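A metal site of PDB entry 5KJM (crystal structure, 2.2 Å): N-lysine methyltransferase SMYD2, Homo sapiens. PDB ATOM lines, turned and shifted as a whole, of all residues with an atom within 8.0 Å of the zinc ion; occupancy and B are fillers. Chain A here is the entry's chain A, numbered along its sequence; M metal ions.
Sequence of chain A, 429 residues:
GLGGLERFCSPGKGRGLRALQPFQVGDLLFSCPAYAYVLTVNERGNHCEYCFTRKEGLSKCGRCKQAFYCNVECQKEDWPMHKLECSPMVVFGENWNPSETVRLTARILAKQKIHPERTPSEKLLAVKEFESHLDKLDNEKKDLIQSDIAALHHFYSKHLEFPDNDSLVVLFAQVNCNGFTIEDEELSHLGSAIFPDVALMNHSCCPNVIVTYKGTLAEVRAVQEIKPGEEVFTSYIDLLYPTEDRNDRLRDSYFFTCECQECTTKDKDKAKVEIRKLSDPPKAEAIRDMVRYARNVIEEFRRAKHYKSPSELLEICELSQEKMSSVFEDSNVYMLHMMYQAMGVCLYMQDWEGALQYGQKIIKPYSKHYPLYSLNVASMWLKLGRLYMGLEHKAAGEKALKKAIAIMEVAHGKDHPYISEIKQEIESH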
ATOM      1  N   HIS A  47      -2.192  19.418 -11.132  1.00  0.00           N
ATOM      2  CA  HIS A  47      -1.832  18.757  -9.863  1.00  0.00           C
ATOM      3  C   HIS A  47      -3.043  18.103  -9.237  1.00  0.00           C
ATOM      4  O   HIS A  47      -4.175  18.559  -9.447  1.00  0.00           O
ATOM      5  CB  HIS A  47      -1.263  19.761  -8.847  1.00  0.00           C
ATOM      6  CG  HIS A  47      -0.040  20.481  -9.300  1.00  0.00           C
ATOM      7  ND1 HIS A  47       1.201  20.184  -8.767  1.00  0.00           N
ATOM      8  CD2 HIS A  47       0.078  21.498 -10.182  1.00  0.00           C
ATOM      9  CE1 HIS A  47       2.037  21.026  -9.354  1.00  0.00           C
ATOM     10  NE2 HIS A  47       1.415  21.822 -10.221  1.00  0.00           N
ATOM     11  N   CYS A  48      -2.812  17.057  -8.444  1.00  0.00           N
ATOM     12  CA  CYS A  48      -3.895  16.425  -7.695  1.00  0.00           C
ATOM     13  C   CYS A  48      -4.326  17.403  -6.599  1.00  0.00           C
ATOM     14  O   CYS A  48      -3.492  18.016  -5.952  1.00  0.00           O
ATOM     15  CB  CYS A  48      -3.480  15.079  -7.118  1.00  0.00           C
ATOM     16  SG  CYS A  48      -4.677  14.400  -5.922  1.00  0.00           S
ATOM     17  N   GLU A  49      -5.632  17.550  -6.448  1.00  0.00           N
ATOM     18  CA  GLU A  49      -6.296  18.436  -5.505  1.00  0.00           C
ATOM     19  C   GLU A  49      -5.961  18.017  -4.048  1.00  0.00           C
ATOM     20  O   GLU A  49      -5.720  18.871  -3.207  1.00  0.00           O
ATOM     21  CB  GLU A  49      -7.804  18.331  -5.784  1.00  0.00           C
ATOM     22  CG  GLU A  49      -8.640  19.509  -5.414  1.00  0.00           C
ATOM     23  CD  GLU A  49      -8.706  20.720  -6.321  1.00  0.00           C
ATOM     24  OE1 GLU A  49      -8.462  20.602  -7.549  1.00  0.00           O
ATOM     25  OE2 GLU A  49      -9.085  21.791  -5.802  1.00  0.00           O
ATOM     26  N   TYR A  50      -5.897  16.696  -3.795  1.00  0.00           N
ATOM     27  CA  TYR A  50      -5.627  16.146  -2.465  1.00  0.00           C
ATOM     28  C   TYR A  50      -4.140  16.142  -2.017  1.00  0.00           C
ATOM     29  O   TYR A  50      -3.848  16.563  -0.896  1.00  0.00           O
ATOM     30  CB  TYR A  50      -6.236  14.735  -2.339  1.00  0.00           C
ATOM     31  CG  TYR A  50      -6.005  14.129  -0.968  1.00  0.00           C
ATOM     32  CD1 TYR A  50      -5.106  13.080  -0.786  1.00  0.00           C
ATOM     33  CD2 TYR A  50      -6.625  14.661   0.161  1.00  0.00           C
ATOM     34  CE1 TYR A  50      -4.866  12.541   0.482  1.00  0.00           C
ATOM     35  CE2 TYR A  50      -6.351  14.170   1.432  1.00  0.00           C
ATOM     36  CZ  TYR A  50      -5.478  13.109   1.590  1.00  0.00           C
ATOM     37  OH  TYR A  50      -5.258  12.591   2.837  1.00  0.00           O
ATOM     38  N   CYS A  51      -3.231  15.598  -2.869  1.00  0.00           N
ATOM     39  CA  CYS A  51      -1.828  15.474  -2.480  1.00  0.00           C
ATOM     40  C   CYS A  51      -0.844  16.421  -3.229  1.00  0.00           C
ATOM     41  O   CYS A  51       0.339  16.400  -2.911  1.00  0.00           O
ATOM     42  CB  CYS A  51      -1.400  14.014  -2.621  1.00  0.00           C
ATOM     43  SG  CYS A  51      -1.293  13.476  -4.338  1.00  0.00           S
ATOM     44  N   PHE A  52      -1.313  17.185  -4.229  1.00  0.00           N
ATOM     45  CA  PHE A  52      -0.497  18.150  -5.008  1.00  0.00           C
ATOM     46  C   PHE A  52       0.560  17.499  -5.924  1.00  0.00           C
ATOM     47  O   PHE A  52       1.484  18.183  -6.357  1.00  0.00           O
ATOM     48  CB  PHE A  52       0.146  19.243  -4.111  1.00  0.00           C
ATOM     49  CG  PHE A  52      -0.723  20.440  -3.734  1.00  0.00           C
ATOM     50  CD1 PHE A  52      -0.167  21.707  -3.637  1.00  0.00           C
ATOM     51  CD2 PHE A  52      -2.074  20.278  -3.437  1.00  0.00           C
ATOM     52  CE1 PHE A  52      -0.956  22.810  -3.257  1.00  0.00           C
ATOM     53  CE2 PHE A  52      -2.854  21.378  -3.039  1.00  0.00           C
ATOM     54  CZ  PHE A  52      -2.283  22.625  -2.930  1.00  0.00           C
ATOM     55  N   THR A  53       0.381  16.204  -6.268  1.00  0.00           N
ATOM     56  CA  THR A  53       1.257  15.480  -7.203  1.00  0.00           C
ATOM     57  C   THR A  53       1.061  16.075  -8.593  1.00  0.00           C
ATOM     58  O   THR A  53      -0.076  16.239  -9.019  1.00  0.00           O
ATOM     59  CB  THR A  53       0.914  13.969  -7.173  1.00  0.00           C
ATOM     60  OG1 THR A  53       1.290  13.468  -5.906  1.00  0.00           O
ATOM     61  CG2 THR A  53       1.610  13.151  -8.286  1.00  0.00           C
ATOM     62  N   ARG A  54       2.164  16.452  -9.262  1.00  0.00           N
ATOM     63  CA  ARG A  54       2.131  16.979 -10.617  1.00  0.00           C
ATOM     64  C   ARG A  54       2.273  15.756 -11.532  1.00  0.00           C
ATOM     65  O   ARG A  54       3.308  15.091 -11.525  1.00  0.00           O
ATOM     66  CB  ARG A  54       3.221  18.034 -10.826  1.00  0.00           C
ATOM     67  CG  ARG A  54       3.143  18.739 -12.185  1.00  0.00           C
ATOM     68  CD  ARG A  54       4.142  19.874 -12.316  1.00  0.00           C
ATOM     69  NE  ARG A  54       5.519  19.443 -12.093  1.00  0.00           N
ATOM     70  CZ  ARG A  54       6.465  20.185 -11.532  1.00  0.00           C
ATOM     71  NH1 ARG A  54       6.195  21.424 -11.112  1.00  0.00           N
ATOM     72  NH2 ARG A  54       7.694  19.700 -11.372  1.00  0.00           N
ATOM     73  N   LYS A  55       1.196  15.417 -12.241  1.00  0.00           N
ATOM     74  CA  LYS A  55       1.090  14.221 -13.093  1.00  0.00           C
ATOM     75  C   LYS A  55       0.224  14.510 -14.315  1.00  0.00           C
ATOM     76  O   LYS A  55      -0.679  15.353 -14.240  1.00  0.00           O
ATOM     77  CB  LYS A  55       0.317  13.160 -12.283  1.00  0.00           C
ATOM     78  CG  LYS A  55       1.034  11.891 -11.888  1.00  0.00           C
ATOM     79  CD  LYS A  55       0.018  10.876 -11.304  1.00  0.00           C
ATOM     80  CE  LYS A  55      -0.886  10.243 -12.345  1.00  0.00           C
ATOM     81  NZ  LYS A  55      -2.078   9.576 -11.753  1.00  0.00           N
ATOM     82  N   LEU A  58      -4.786  12.925 -14.823  1.00  0.00           N
ATOM     83  CA  LEU A  58      -5.492  12.991 -13.546  1.00  0.00           C
ATOM     84  C   LEU A  58      -6.998  12.789 -13.809  1.00  0.00           C
ATOM     85  O   LEU A  58      -7.498  13.258 -14.835  1.00  0.00           O
ATOM     86  CB  LEU A  58      -5.262  14.343 -12.837  1.00  0.00           C
ATOM     87  CG  LEU A  58      -3.861  14.640 -12.274  1.00  0.00           C
ATOM     88  CD1 LEU A  58      -3.715  16.117 -11.962  1.00  0.00           C
ATOM     89  CD2 LEU A  58      -3.570  13.809 -11.036  1.00  0.00           C
ATOM     90  N   PHE A  68      -9.328  17.733  -9.891  1.00  0.00           N
ATOM     91  CA  PHE A  68      -8.608  16.620 -10.508  1.00  0.00           C
ATOM     92  C   PHE A  68      -7.803  15.850  -9.464  1.00  0.00           C
ATOM     93  O   PHE A  68      -7.236  16.448  -8.541  1.00  0.00           O
ATOM     94  CB  PHE A  68      -7.759  17.072 -11.727  1.00  0.00           C
ATOM     95  CG  PHE A  68      -8.560  17.679 -12.857  1.00  0.00           C
ATOM     96  CD1 PHE A  68      -8.818  16.949 -14.014  1.00  0.00           C
ATOM     97  CD2 PHE A  68      -9.070  18.973 -12.774  1.00  0.00           C
ATOM     98  CE1 PHE A  68      -9.553  17.511 -15.071  1.00  0.00           C
ATOM     99  CE2 PHE A  68      -9.801  19.534 -13.822  1.00  0.00           C
ATOM    100  CZ  PHE A  68     -10.038  18.804 -14.955  1.00  0.00           C
ATOM    101  N   TYR A  69      -7.822  14.505  -9.579  1.00  0.00           N
ATOM    102  CA  TYR A  69      -7.226  13.589  -8.609  1.00  0.00           C
ATOM    103  C   TYR A  69      -6.358  12.495  -9.225  1.00  0.00           C
ATOM    104  O   TYR A  69      -6.597  12.094 -10.367  1.00  0.00           O
ATOM    105  CB  TYR A  69      -8.344  12.952  -7.766  1.00  0.00           C
ATOM    106  CG  TYR A  69      -9.204  13.959  -7.035  1.00  0.00           C
ATOM    107  CD1 TYR A  69     -10.422  14.383  -7.568  1.00  0.00           C
ATOM    108  CD2 TYR A  69      -8.786  14.523  -5.836  1.00  0.00           C
ATOM    109  CE1 TYR A  69     -11.219  15.311  -6.892  1.00  0.00           C
ATOM    110  CE2 TYR A  69      -9.591  15.417  -5.140  1.00  0.00           C
ATOM    111  CZ  TYR A  69     -10.793  15.828  -5.682  1.00  0.00           C
ATOM    112  OH  TYR A  69     -11.549  16.742  -4.982  1.00  0.00           O
ATOM    113  N   CYS A  70      -5.388  11.968  -8.438  1.00  0.00           N
ATOM    114  CA  CYS A  70      -4.507  10.857  -8.840  1.00  0.00           C
ATOM    115  C   CYS A  70      -5.338   9.625  -9.172  1.00  0.00           C
ATOM    116  O   CYS A  70      -5.119   8.975 -10.190  1.00  0.00           O
ATOM    117  CB  CYS A  70      -3.496  10.532  -7.747  1.00  0.00           C
ATOM    118  SG  CYS A  70      -2.296  11.853  -7.460  1.00  0.00           S
ATOM    119  N   ASN A  71      -6.301   9.331  -8.285  1.00  0.00           N
ATOM    120  CA  ASN A  71      -7.181   8.168  -8.337  1.00  0.00           C
ATOM    121  C   ASN A  71      -8.410   8.429  -7.453  1.00  0.00           C
ATOM    122  O   ASN A  71      -8.572   9.525  -6.930  1.00  0.00           O
ATOM    123  CB  ASN A  71      -6.397   6.927  -7.846  1.00  0.00           C
ATOM    124  CG  ASN A  71      -5.609   7.191  -6.580  1.00  0.00           C
ATOM    125  OD1 ASN A  71      -6.125   7.693  -5.584  1.00  0.00           O
ATOM    126  ND2 ASN A  71      -4.333   6.895  -6.621  1.00  0.00           N
ATOM    127  N   GLU A  73      -8.944   7.208  -4.461  1.00  0.00           N
ATOM    128  CA  GLU A  73      -8.536   7.377  -3.058  1.00  0.00           C
ATOM    129  C   GLU A  73      -8.268   8.830  -2.751  1.00  0.00           C
ATOM    130  O   GLU A  73      -8.829   9.340  -1.765  1.00  0.00           O
ATOM    131  CB  GLU A  73      -7.305   6.514  -2.697  1.00  0.00           C
ATOM    132  CG  GLU A  73      -7.668   5.111  -2.216  1.00  0.00           C
ATOM    133  CD  GLU A  73      -8.414   4.224  -3.196  1.00  0.00           C
ATOM    134  OE1 GLU A  73      -9.586   3.877  -2.903  1.00  0.00           O
ATOM    135  OE2 GLU A  73      -7.853   3.911  -4.270  1.00  0.00           O
ATOM    136  N   CYS A  74      -7.463   9.525  -3.595  1.00  0.00           N
ATOM    137  CA  CYS A  74      -7.181  10.955  -3.453  1.00  0.00           C
ATOM    138  C   CYS A  74      -8.524  11.743  -3.508  1.00  0.00           C
ATOM    139  O   CYS A  74      -8.744  12.644  -2.690  1.00  0.00           O
ATOM    140  CB  CYS A  74      -6.203  11.420  -4.529  1.00  0.00           C
ATOM    141  SG  CYS A  74      -4.441  11.127  -4.125  1.00  0.00           S
ATOM    142  N   GLN A  75      -9.446  11.320  -4.392  1.00  0.00           N
ATOM    143  CA  GLN A  75     -10.775  11.898  -4.546  1.00  0.00           C
ATOM    144  C   GLN A  75     -11.620  11.793  -3.257  1.00  0.00           C
ATOM    145  O   GLN A  75     -12.127  12.818  -2.798  1.00  0.00           O
ATOM    146  CB  GLN A  75     -11.497  11.314  -5.775  1.00  0.00           C
ATOM    147  CG  GLN A  75     -12.837  11.995  -6.061  1.00  0.00           C
ATOM    148  CD  GLN A  75     -13.515  11.576  -7.338  1.00  0.00           C
ATOM    149  OE1 GLN A  75     -14.606  12.058  -7.663  1.00  0.00           O
ATOM    150  NE2 GLN A  75     -12.902  10.680  -8.102  1.00  0.00           N
HETATM  151 ZN    ZN M   1      -3.268  12.611  -5.359  1.00  0.00          ZN
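SG of Cys 74 is bound to the zinc ion (2.3 Å).
SG of Cys 48 binds the zinc ion (2.3 Å).
SG of Cys 51 is bound to the zinc ion (2.4 Å).
The zinc ion is bound by SG of Cys 70 (2.4 Å).
The backbone NH of Tyr 50 lies close to the side-chain sulfur of Cys 48, at 3.4 Å.
SG of Cys 51 lies close to OG1 of Thr 53 (3.0 Å).
N of Cys 48 lies within hydrogen-bond range of O of Thr 53 (2.9 Å).
The side-chain amino group (NZ) of Lys 55 is in hydrogen-bond range of the backbone carbonyl oxygen (O) of Cys 70.
N of Cys 74 sits at hydrogen-bond distance from OD1 of Asn 71 (3.0 Å).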
